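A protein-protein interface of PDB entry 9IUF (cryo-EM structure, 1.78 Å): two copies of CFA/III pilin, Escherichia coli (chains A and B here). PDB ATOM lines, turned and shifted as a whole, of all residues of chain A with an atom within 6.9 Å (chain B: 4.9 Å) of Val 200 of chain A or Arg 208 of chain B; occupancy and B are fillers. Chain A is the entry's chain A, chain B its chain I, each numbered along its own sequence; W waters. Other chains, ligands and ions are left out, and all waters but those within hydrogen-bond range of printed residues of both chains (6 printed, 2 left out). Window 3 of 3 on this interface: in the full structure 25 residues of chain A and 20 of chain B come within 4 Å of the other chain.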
ATOM      1  N   GLN A  25      -8.915  -9.637  -7.759  1.00  0.00           N
ATOM      2  CA  GLN A  25      -9.101 -10.388  -6.520  1.00  0.00           C
ATOM      3  C   GLN A  25      -9.202 -11.886  -6.793  1.00  0.00           C
ATOM      4  O   GLN A  25      -8.577 -12.699  -6.096  1.00  0.00           O
ATOM      5  CB  GLN A  25     -10.342  -9.889  -5.781  1.00  0.00           C
ATOM      6  CG  GLN A  25     -10.607 -10.597  -4.462  1.00  0.00           C
ATOM      7  CD  GLN A  25      -9.396 -10.614  -3.550  1.00  0.00           C
ATOM      8  OE1 GLN A  25      -9.032 -11.654  -3.006  1.00  0.00           O
ATOM      9  NE2 GLN A  25      -8.766  -9.459  -3.377  1.00  0.00           N
ATOM     10  N   PHE A  28      -5.739 -13.327  -7.670  1.00  0.00           N
ATOM     11  CA  PHE A  28      -4.920 -13.501  -6.475  1.00  0.00           C
ATOM     12  C   PHE A  28      -5.356 -14.734  -5.694  1.00  0.00           C
ATOM     13  O   PHE A  28      -4.514 -15.516  -5.234  1.00  0.00           O
ATOM     14  CB  PHE A  28      -4.993 -12.256  -5.592  1.00  0.00           C
ATOM     15  CG  PHE A  28      -4.302 -12.412  -4.264  1.00  0.00           C
ATOM     16  CD1 PHE A  28      -2.947 -12.160  -4.142  1.00  0.00           C
ATOM     17  CD2 PHE A  28      -5.005 -12.816  -3.141  1.00  0.00           C
ATOM     18  CE1 PHE A  28      -2.307 -12.304  -2.927  1.00  0.00           C
ATOM     19  CE2 PHE A  28      -4.368 -12.967  -1.925  1.00  0.00           C
ATOM     20  CZ  PHE A  28      -3.018 -12.707  -1.818  1.00  0.00           C
ATOM     21  N   GLY A  97       0.287 -17.928   1.927  1.00  0.00           N
ATOM     22  CA  GLY A  97       0.165 -16.721   1.130  1.00  0.00           C
ATOM     23  C   GLY A  97      -1.108 -15.936   1.363  1.00  0.00           C
ATOM     24  O   GLY A  97      -1.200 -14.794   0.903  1.00  0.00           O
ATOM     25  N   ILE A  98      -2.080 -16.515   2.058  1.00  0.00           N
ATOM     26  CA  ILE A  98      -3.337 -15.825   2.332  1.00  0.00           C
ATOM     27  C   ILE A  98      -3.296 -15.112   3.676  1.00  0.00           C
ATOM     28  O   ILE A  98      -3.612 -13.923   3.769  1.00  0.00           O
ATOM     29  CB  ILE A  98      -4.508 -16.826   2.256  1.00  0.00           C
ATOM     30  CG1 ILE A  98      -4.670 -17.337   0.823  1.00  0.00           C
ATOM     31  CG2 ILE A  98      -5.792 -16.182   2.748  1.00  0.00           C
ATOM     32  CD1 ILE A  98      -5.630 -18.491   0.688  1.00  0.00           C
ATOM     33  N   SER A  99      -2.906 -15.819   4.734  1.00  0.00           N
ATOM     34  CA  SER A  99      -2.854 -15.230   6.065  1.00  0.00           C
ATOM     35  C   SER A  99      -1.536 -14.531   6.362  1.00  0.00           C
ATOM     36  O   SER A  99      -1.482 -13.712   7.285  1.00  0.00           O
ATOM     37  CB  SER A  99      -3.098 -16.307   7.126  1.00  0.00           C
ATOM     38  OG  SER A  99      -2.055 -17.264   7.127  1.00  0.00           O
ATOM     39  N   ASN A 125      -4.722 -21.082   8.077  1.00  0.00           N
ATOM     40  CA  ASN A 125      -5.645 -20.187   8.757  1.00  0.00           C
ATOM     41  C   ASN A 125      -5.932 -18.951   7.910  1.00  0.00           C
ATOM     42  O   ASN A 125      -5.289 -18.695   6.891  1.00  0.00           O
ATOM     43  CB  ASN A 125      -5.082 -19.776  10.120  1.00  0.00           C
ATOM     44  CG  ASN A 125      -3.718 -19.123  10.013  1.00  0.00           C
ATOM     45  OD1 ASN A 125      -3.081 -19.157   8.961  1.00  0.00           O
ATOM     46  ND2 ASN A 125      -3.262 -18.523  11.104  1.00  0.00           N
ATOM     47  N   GLY A 126      -6.927 -18.183   8.351  1.00  0.00           N
ATOM     48  CA  GLY A 126      -7.249 -16.924   7.713  1.00  0.00           C
ATOM     49  C   GLY A 126      -7.876 -17.035   6.344  1.00  0.00           C
ATOM     50  O   GLY A 126      -7.841 -16.068   5.580  1.00  0.00           O
ATOM     51  N   LEU A 127      -8.455 -18.183   6.010  1.00  0.00           N
ATOM     52  CA  LEU A 127      -9.024 -18.384   4.687  1.00  0.00           C
ATOM     53  C   LEU A 127     -10.413 -17.769   4.591  1.00  0.00           C
ATOM     54  O   LEU A 127     -11.220 -17.869   5.519  1.00  0.00           O
ATOM     55  CB  LEU A 127      -9.100 -19.874   4.357  1.00  0.00           C
ATOM     56  CG  LEU A 127      -7.842 -20.702   4.606  1.00  0.00           C
ATOM     57  CD1 LEU A 127      -8.125 -22.173   4.363  1.00  0.00           C
ATOM     58  CD2 LEU A 127      -6.708 -20.219   3.725  1.00  0.00           C
ATOM     59  N   SER A 128     -10.686 -17.126   3.461  1.00  0.00           N
ATOM     60  CA  SER A 128     -12.040 -16.694   3.166  1.00  0.00           C
ATOM     61  C   SER A 128     -12.896 -17.899   2.789  1.00  0.00           C
ATOM     62  O   SER A 128     -12.401 -19.008   2.573  1.00  0.00           O
ATOM     63  CB  SER A 128     -12.040 -15.660   2.041  1.00  0.00           C
ATOM     64  OG  SER A 128     -11.863 -16.280   0.779  1.00  0.00           O
ATOM     65  N   GLN A 129     -14.209 -17.674   2.720  1.00  0.00           N
ATOM     66  CA  GLN A 129     -15.116 -18.752   2.342  1.00  0.00           C
ATOM     67  C   GLN A 129     -14.807 -19.263   0.941  1.00  0.00           C
ATOM     68  O   GLN A 129     -14.761 -20.478   0.707  1.00  0.00           O
ATOM     69  CB  GLN A 129     -16.563 -18.271   2.434  1.00  0.00           C
ATOM     70  CG  GLN A 129     -17.587 -19.288   1.980  1.00  0.00           C
ATOM     71  CD  GLN A 129     -19.002 -18.874   2.328  1.00  0.00           C
ATOM     72  OE1 GLN A 129     -19.602 -18.045   1.647  1.00  0.00           O
ATOM     73  NE2 GLN A 129     -19.541 -19.450   3.394  1.00  0.00           N
ATOM     74  N   GLU A 130     -14.570 -18.346   0.000  1.00  0.00           N
ATOM     75  CA  GLU A 130     -14.242 -18.745  -1.364  1.00  0.00           C
ATOM     76  C   GLU A 130     -12.940 -19.533  -1.402  1.00  0.00           C
ATOM     77  O   GLU A 130     -12.852 -20.573  -2.064  1.00  0.00           O
ATOM     78  CB  GLU A 130     -14.152 -17.511  -2.264  1.00  0.00           C
ATOM     79  CG  GLU A 130     -15.445 -16.717  -2.381  1.00  0.00           C
ATOM     80  CD  GLU A 130     -15.652 -15.747  -1.231  1.00  0.00           C
ATOM     81  OE1 GLU A 130     -16.670 -15.025  -1.239  1.00  0.00           O
ATOM     82  OE2 GLU A 130     -14.797 -15.703  -0.322  1.00  0.00           O
ATOM     83  N   GLN A 131     -11.917 -19.055  -0.691  1.00  0.00           N
ATOM     84  CA  GLN A 131     -10.642 -19.766  -0.657  1.00  0.00           C
ATOM     85  C   GLN A 131     -10.783 -21.122   0.023  1.00  0.00           C
ATOM     86  O   GLN A 131     -10.205 -22.113  -0.437  1.00  0.00           O
ATOM     87  CB  GLN A 131      -9.586 -18.919   0.050  1.00  0.00           C
ATOM     88  CG  GLN A 131      -9.136 -17.706  -0.743  1.00  0.00           C
ATOM     89  CD  GLN A 131      -8.699 -16.561   0.146  1.00  0.00           C
ATOM     90  OE1 GLN A 131      -8.810 -16.632   1.368  1.00  0.00           O
ATOM     91  NE2 GLN A 131      -8.198 -15.496  -0.465  1.00  0.00           N
ATOM     92  N   GLY A 149     -12.157 -25.482  10.475  1.00  0.00           N
ATOM     93  CA  GLY A 149     -12.352 -24.706  11.683  1.00  0.00           C
ATOM     94  C   GLY A 149     -12.453 -23.223  11.395  1.00  0.00           C
ATOM     95  O   GLY A 149     -12.699 -22.823  10.254  1.00  0.00           O
ATOM     96  N   THR A 150     -12.252 -22.392  12.419  1.00  0.00           N
ATOM     97  CA  THR A 150     -12.395 -20.948  12.281  1.00  0.00           C
ATOM     98  C   THR A 150     -11.166 -20.210  12.798  1.00  0.00           C
ATOM     99  O   THR A 150     -11.284 -19.120  13.363  1.00  0.00           O
ATOM    100  CB  THR A 150     -13.647 -20.451  13.004  1.00  0.00           C
ATOM    101  OG1 THR A 150     -13.637 -20.920  14.358  1.00  0.00           O
ATOM    102  CG2 THR A 150     -14.903 -20.954  12.308  1.00  0.00           C
ATOM    103  N   SER A 151      -9.984 -20.782  12.616  1.00  0.00           N
ATOM    104  CA  SER A 151      -8.764 -20.127  13.073  1.00  0.00           C
ATOM    105  C   SER A 151      -8.453 -18.934  12.180  1.00  0.00           C
ATOM    106  O   SER A 151      -8.277 -19.110  10.968  1.00  0.00           O
ATOM    107  CB  SER A 151      -7.595 -21.106  13.072  1.00  0.00           C
ATOM    108  OG  SER A 151      -7.866 -22.227  13.893  1.00  0.00           O
ATOM    109  N   PRO A 152      -8.374 -17.726  12.717  1.00  0.00           N
ATOM    110  CA  PRO A 152      -8.071 -16.553  11.896  1.00  0.00           C
ATOM    111  C   PRO A 152      -6.570 -16.435  11.654  1.00  0.00           C
ATOM    112  O   PRO A 152      -5.771 -17.226  12.149  1.00  0.00           O
ATOM    113  CB  PRO A 152      -8.596 -15.397  12.746  1.00  0.00           C
ATOM    114  CG  PRO A 152      -8.415 -15.873  14.145  1.00  0.00           C
ATOM    115  CD  PRO A 152      -8.621 -17.366  14.124  1.00  0.00           C
ATOM    116  N   SER A 153      -6.201 -15.427  10.869  1.00  0.00           N
ATOM    117  CA  SER A 153      -4.791 -15.149  10.629  1.00  0.00           C
ATOM    118  C   SER A 153      -4.098 -14.807  11.942  1.00  0.00           C
ATOM    119  O   SER A 153      -4.607 -14.013  12.738  1.00  0.00           O
ATOM    120  CB  SER A 153      -4.641 -14.002   9.632  1.00  0.00           C
ATOM    121  OG  SER A 153      -5.385 -14.247   8.452  1.00  0.00           O
ATOM    122  N   THR A 197     -18.584 -22.273   6.362  1.00  0.00           N
ATOM    123  CA  THR A 197     -19.759 -21.419   6.494  1.00  0.00           C
ATOM    124  C   THR A 197     -19.448 -20.021   7.010  1.00  0.00           C
ATOM    125  O   THR A 197     -20.297 -19.133   6.882  1.00  0.00           O
ATOM    126  CB  THR A 197     -20.784 -22.080   7.420  1.00  0.00           C
ATOM    127  OG1 THR A 197     -20.180 -22.339   8.694  1.00  0.00           O
ATOM    128  CG2 THR A 197     -21.272 -23.388   6.822  1.00  0.00           C
ATOM    129  N   ALA A 198     -18.272 -19.796   7.583  1.00  0.00           N
ATOM    130  CA  ALA A 198     -17.917 -18.498   8.134  1.00  0.00           C
ATOM    131  C   ALA A 198     -17.137 -17.674   7.116  1.00  0.00           C
ATOM    132  O   ALA A 198     -16.627 -18.187   6.117  1.00  0.00           O
ATOM    133  CB  ALA A 198     -17.107 -18.665   9.422  1.00  0.00           C
ATOM    134  N   THR A 199     -17.053 -16.369   7.381  1.00  0.00           N
ATOM    135  CA  THR A 199     -16.248 -15.494   6.535  1.00  0.00           C
ATOM    136  C   THR A 199     -14.759 -15.716   6.752  1.00  0.00           C
ATOM    137  O   THR A 199     -13.962 -15.484   5.837  1.00  0.00           O
ATOM    138  CB  THR A 199     -16.601 -14.030   6.794  1.00  0.00           C
ATOM    139  OG1 THR A 199     -16.324 -13.702   8.161  1.00  0.00           O
ATOM    140  CG2 THR A 199     -18.070 -13.776   6.505  1.00  0.00           C
ATOM    141  N   VAL A 200     -14.369 -16.157   7.943  1.00  0.00           N
ATOM    142  CA  VAL A 200     -12.992 -16.524   8.246  1.00  0.00           C
ATOM    143  C   VAL A 200     -12.982 -18.007   8.585  1.00  0.00           C
ATOM    144  O   VAL A 200     -13.650 -18.436   9.533  1.00  0.00           O
ATOM    145  CB  VAL A 200     -12.414 -15.691   9.399  1.00  0.00           C
ATOM    146  CG1 VAL A 200     -11.016 -16.167   9.742  1.00  0.00           C
ATOM    147  CG2 VAL A 200     -12.404 -14.217   9.032  1.00  0.00           C
ATOM    148  N   ASN A 201     -12.226 -18.785   7.816  1.00  0.00           N
ATOM    149  CA  ASN A 201     -12.184 -20.228   7.974  1.00  0.00           C
ATOM    150  C   ASN A 201     -10.740 -20.701   8.002  1.00  0.00           C
ATOM    151  O   ASN A 201      -9.821 -19.992   7.582  1.00  0.00           O
ATOM    152  CB  ASN A 201     -12.939 -20.944   6.844  1.00  0.00           C
ATOM    153  CG  ASN A 201     -14.341 -20.407   6.649  1.00  0.00           C
ATOM    154  OD1 ASN A 201     -15.291 -20.885   7.267  1.00  0.00           O
ATOM    155  ND2 ASN A 201     -14.478 -19.412   5.784  1.00  0.00           N
ATOM    156  N   SER A 202     -10.550 -21.913   8.512  1.00  0.00           N
ATOM    157  CA  SER A 202      -9.248 -22.560   8.507  1.00  0.00           C
ATOM    158  C   SER A 202      -9.428 -24.016   8.111  1.00  0.00           C
ATOM    159  O   SER A 202     -10.490 -24.606   8.307  1.00  0.00           O
ATOM    160  CB  SER A 202      -8.558 -22.461   9.873  1.00  0.00           C
ATOM    161  OG  SER A 202      -9.281 -23.174  10.859  1.00  0.00           O
ATOM    162  N   LYS B  48      -0.898  -5.639  -1.315  1.00  0.00           N
ATOM    163  CA  LYS B  48      -0.882  -7.084  -1.129  1.00  0.00           C
ATOM    164  C   LYS B  48       0.443  -7.679  -1.588  1.00  0.00           C
ATOM    165  O   LYS B  48       0.975  -8.596  -0.949  1.00  0.00           O
ATOM    166  CB  LYS B  48      -2.053  -7.716  -1.876  1.00  0.00           C
ATOM    167  CG  LYS B  48      -3.290  -7.888  -1.017  1.00  0.00           C
ATOM    168  CD  LYS B  48      -4.537  -8.006  -1.872  1.00  0.00           C
ATOM    169  CE  LYS B  48      -4.840  -9.450  -2.202  1.00  0.00           C
ATOM    170  NZ  LYS B  48      -5.127 -10.222  -0.963  1.00  0.00           N
ATOM    171  N   TYR B  57       0.714  -5.721   7.858  1.00  0.00           N
ATOM    172  CA  TYR B  57       0.705  -4.474   7.120  1.00  0.00           C
ATOM    173  C   TYR B  57       1.072  -3.305   8.029  1.00  0.00           C
ATOM    174  O   TYR B  57       0.792  -3.335   9.231  1.00  0.00           O
ATOM    175  CB  TYR B  57      -0.669  -4.238   6.483  1.00  0.00           C
ATOM    176  CG  TYR B  57      -0.995  -5.261   5.420  1.00  0.00           C
ATOM    177  CD1 TYR B  57      -0.469  -5.152   4.142  1.00  0.00           C
ATOM    178  CD2 TYR B  57      -1.811  -6.347   5.702  1.00  0.00           C
ATOM    179  CE1 TYR B  57      -0.755  -6.088   3.170  1.00  0.00           C
ATOM    180  CE2 TYR B  57      -2.103  -7.287   4.737  1.00  0.00           C
ATOM    181  CZ  TYR B  57      -1.573  -7.153   3.472  1.00  0.00           C
ATOM    182  OH  TYR B  57      -1.863  -8.088   2.508  1.00  0.00           O
ATOM    183  N   THR B 110      -8.352  -8.631  11.280  1.00  0.00           N
ATOM    184  CA  THR B 110      -9.284  -9.572  10.675  1.00  0.00           C
ATOM    185  C   THR B 110      -9.858 -10.554  11.690  1.00  0.00           C
ATOM    186  O   THR B 110     -10.421 -11.583  11.303  1.00  0.00           O
ATOM    187  CB  THR B 110      -8.608 -10.328   9.532  1.00  0.00           C
ATOM    188  OG1 THR B 110      -7.450 -11.010  10.028  1.00  0.00           O
ATOM    189  CG2 THR B 110      -8.188  -9.365   8.435  1.00  0.00           C
ATOM    190  N   LYS B 118      -3.392  -7.757  10.041  1.00  0.00           N
ATOM    191  CA  LYS B 118      -3.436  -8.784   9.011  1.00  0.00           C
ATOM    192  C   LYS B 118      -4.161  -8.324   7.755  1.00  0.00           C
ATOM    193  O   LYS B 118      -4.131  -9.034   6.744  1.00  0.00           O
ATOM    194  CB  LYS B 118      -4.095 -10.050   9.559  1.00  0.00           C
ATOM    195  CG  LYS B 118      -3.189 -10.850  10.475  1.00  0.00           C
ATOM    196  CD  LYS B 118      -1.873 -11.175   9.789  1.00  0.00           C
ATOM    197  CE  LYS B 118      -1.118 -12.266  10.526  1.00  0.00           C
ATOM    198  NZ  LYS B 118       0.044 -12.758   9.738  1.00  0.00           N
ATOM    199  N   GLY B 119      -4.813  -7.162   7.797  1.00  0.00           N
ATOM    200  CA  GLY B 119      -5.374  -6.546   6.615  1.00  0.00           C
ATOM    201  C   GLY B 119      -4.998  -5.077   6.561  1.00  0.00           C
ATOM    202  O   GLY B 119      -4.352  -4.548   7.466  1.00  0.00           O
ATOM    203  N   GLU B 144     -14.393  -6.067   0.606  1.00  0.00           N
ATOM    204  CA  GLU B 144     -14.910  -6.851   1.722  1.00  0.00           C
ATOM    205  C   GLU B 144     -15.391  -5.959   2.860  1.00  0.00           C
ATOM    206  O   GLU B 144     -16.440  -6.226   3.456  1.00  0.00           O
ATOM    207  CB  GLU B 144     -13.852  -7.837   2.212  1.00  0.00           C
ATOM    208  CG  GLU B 144     -14.074  -9.253   1.703  1.00  0.00           C
ATOM    209  CD  GLU B 144     -12.881 -10.156   1.935  1.00  0.00           C
ATOM    210  OE1 GLU B 144     -11.740  -9.651   1.927  1.00  0.00           O
ATOM    211  OE2 GLU B 144     -13.085 -11.373   2.126  1.00  0.00           O
ATOM    212  N   MET B 166     -12.327  -4.932  10.934  1.00  0.00           N
ATOM    213  CA  MET B 166     -13.056  -5.485   9.801  1.00  0.00           C
ATOM    214  C   MET B 166     -14.209  -6.386  10.219  1.00  0.00           C
ATOM    215  O   MET B 166     -15.042  -6.729   9.374  1.00  0.00           O
ATOM    216  CB  MET B 166     -12.100  -6.258   8.891  1.00  0.00           C
ATOM    217  CG  MET B 166     -11.180  -5.374   8.067  1.00  0.00           C
ATOM    218  SD  MET B 166     -10.094  -6.318   6.981  1.00  0.00           S
ATOM    219  CE  MET B 166     -11.203  -6.675   5.624  1.00  0.00           C
ATOM    220  N   LEU B 179     -16.671  -8.221   7.478  1.00  0.00           N
ATOM    221  CA  LEU B 179     -16.485  -9.659   7.607  1.00  0.00           C
ATOM    222  C   LEU B 179     -17.386 -10.280   8.666  1.00  0.00           C
ATOM    223  O   LEU B 179     -17.349 -11.501   8.847  1.00  0.00           O
ATOM    224  CB  LEU B 179     -15.024  -9.974   7.931  1.00  0.00           C
ATOM    225  CG  LEU B 179     -13.995  -9.560   6.879  1.00  0.00           C
ATOM    226  CD1 LEU B 179     -12.592  -9.925   7.330  1.00  0.00           C
ATOM    227  CD2 LEU B 179     -14.315 -10.200   5.540  1.00  0.00           C
ATOM    228  N   ALA B 206     -11.539  -1.562   3.267  1.00  0.00           N
ATOM    229  CA  ALA B 206     -10.577  -2.444   3.907  1.00  0.00           C
ATOM    230  C   ALA B 206     -10.634  -3.828   3.285  1.00  0.00           C
ATOM    231  O   ALA B 206     -11.716  -4.353   2.987  1.00  0.00           O
ATOM    232  CB  ALA B 206     -10.811  -2.542   5.416  1.00  0.00           C
ATOM    233  N   SER B 207      -9.449  -4.411   3.111  1.00  0.00           N
ATOM    234  CA  SER B 207      -9.268  -5.720   2.508  1.00  0.00           C
ATOM    235  C   SER B 207      -8.271  -6.507   3.344  1.00  0.00           C
ATOM    236  O   SER B 207      -7.535  -5.947   4.160  1.00  0.00           O
ATOM    237  CB  SER B 207      -8.780  -5.607   1.058  1.00  0.00           C
ATOM    238  OG  SER B 207      -8.085  -6.774   0.658  1.00  0.00           O
ATOM    239  N   ARG B 208      -8.269  -7.820   3.148  1.00  0.00           N
ATOM    240  CA  ARG B 208      -7.336  -8.689   3.854  1.00  0.00           C
ATOM    241  C   ARG B 208      -6.364  -9.346   2.880  1.00  0.00           C
ATOM    242  O   ARG B 208      -6.628  -9.428   1.681  1.00  0.00           O
ATOM    243  CB  ARG B 208      -8.088  -9.756   4.651  1.00  0.00           C
ATOM    244  CG  ARG B 208      -9.312 -10.306   3.948  1.00  0.00           C
ATOM    245  CD  ARG B 208      -9.869 -11.513   4.678  1.00  0.00           C
ATOM    246  NE  ARG B 208     -11.173 -11.909   4.157  1.00  0.00           N
ATOM    247  CZ  ARG B 208     -11.878 -12.937   4.605  1.00  0.00           C
ATOM    248  NH1 ARG B 208     -11.432 -13.707   5.583  1.00  0.00           N
ATOM    249  NH2 ARG B 208     -13.061 -13.198   4.058  1.00  0.00           N
ATOM    250  OXT ARG B 208      -5.292  -9.807   3.268  1.00  0.00           O
HETATM  251  O   HOH W   1     -17.592 -13.442  10.834  1.00  0.00           O
HETATM  252  O   HOH W   2     -15.448 -15.040   2.924  1.00  0.00           O
HETATM  253  O   HOH W   3      -8.770 -13.601   6.987  1.00  0.00           O
HETATM  254  O   HOH W   4      -8.488 -13.724   9.604  1.00  0.00           O
HETATM  255  O   HOH W   5      -6.420 -11.950  12.385  1.00  0.00           O
HETATM  256  O   HOH W   6      -6.309 -12.298   7.048  1.00  0.00           O
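The side-chain hydroxyl of Ser 128 of chain A sits at hydrogen-bond distance from the side-chain carboxylate of Glu 130 of chain A, at 3.2 Å.
The side-chain amino group (NZ) of Lys 48 of chain B lies within salt-bridge range of the chain-end carboxylate (O) of Arg 208 of chain B (3.1 Å).
OE2 of Glu 144 of chain B lies within salt-bridge range of NH2 of Arg 208 of chain B (2.7 Å).
N of Leu 179 of chain B sits at hydrogen-bond distance from O of Met 166 of chain B (2.9 Å).
The side-chain hydroxyl (OG) of Ser 99 of chain A sits at hydrogen-bond distance from the side-chain amide oxygen (OD1) of Asn 125 of chain A (2.8 Å).
The side-chain amide oxygen of Gln 131 of chain A is in hydrogen-bond range of the backbone NH of Ser 128 of chain A.
No position is printed for both chains.
Hydrophobic or aromatic side chains of chain A that line the printed part of chain B: Phe 28 and Val 200.
Among the printed residues, 7 pairs touch across the chains.
Among the printed residues, no Asp or Glu carboxylate lies within 4 Å of a Lys or Arg side-chain nitrogen of the other chain.
Water W6 lies within hydrogen-bond range of the side-chain hydroxyl (OG) of Ser 153 of chain A (2.6 Å) and the side-chain hydroxyl (OG1) of Thr 110 of chain B (3.4 Å).
Water W5 bridges the side-chain hydroxyl of Thr 110 of chain B (2.7 Å) and the backbone carbonyl oxygen of Ser 153 of chain A (2.8 Å).
Water W1 bridges O of Leu 179 of chain B and OG1 of Thr 199 of chain A.
Water W2 lies within hydrogen-bond range of the backbone NH (N) of Gln 129 of chain A (2.9 Å), the guanidinium group (NH2) of Arg 208 of chain B (3.2 Å), the backbone carbonyl oxygen (O) of Thr 199 of chain A (3.3 Å) and the side-chain carboxylate (OE2) of Glu 130 of chain A (3.4 Å).
Water W4 bridges OG1 of Thr 110 of chain B (2.9 Å) and N of Ser 153 of chain A (3.1 Å).
Water W3 lies within hydrogen-bond range of the backbone carbonyl oxygen of Gly 126 of chain A (3.0 Å) and the guanidinium group of Arg 208 of chain B (3.0 Å).
The side-chain hydroxyl (OG1) of Thr 199 of chain A sits at hydrogen-bond distance from the backbone carbonyl oxygen (O) of Leu 179 of chain B, at 2.5 Å.
O of Thr 199 of chain A is in hydrogen-bond range of NH2 of Arg 208 of chain B.
The backbone carbonyl oxygen (O) of Ser 99 of chain A sits at hydrogen-bond distance from the side-chain amino group (NZ) of Lys 118 of chain B.
Of the printed residues of chain B, Phe 28 of chain A touches Lys 48 (3.0 Å).
Gln 129 of chain A touches none of the printed residues of chain B.
Ala 198 of chain A touches none of the printed residues of chain B.
Of the printed residues of chain B, Val 200 of chain A touches Arg 208 (3.6 Å).
Of the printed residues of chain A, Lys 48 of chain B touches Phe 28 (3.0 Å).
Of the printed residues of chain A, Lys 118 of chain B touches Ser 99 and Ser 153.
Of the printed residues of chain A, Leu 179 of chain B touches Thr 199.
Of chain A, only Ser 128 (3.3 Å), Thr 199 (3.0 Å) and Val 200 (3.6 Å) come within 4 Å of Arg 208 of chain B.
The nearest printed residue of chain B that does not touch Val 200 of chain A is Thr 110 of chain B (4.003 Å).
Among the printed residues, pairs that only touch across the chains: Phe 28 of chain A with Lys 48 of chain B, Ser 128 of chain A with Arg 208 of chain B, Ser 153 of chain A with Lys 118 of chain B and Val 200 of chain A with Arg 208 of chain B.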
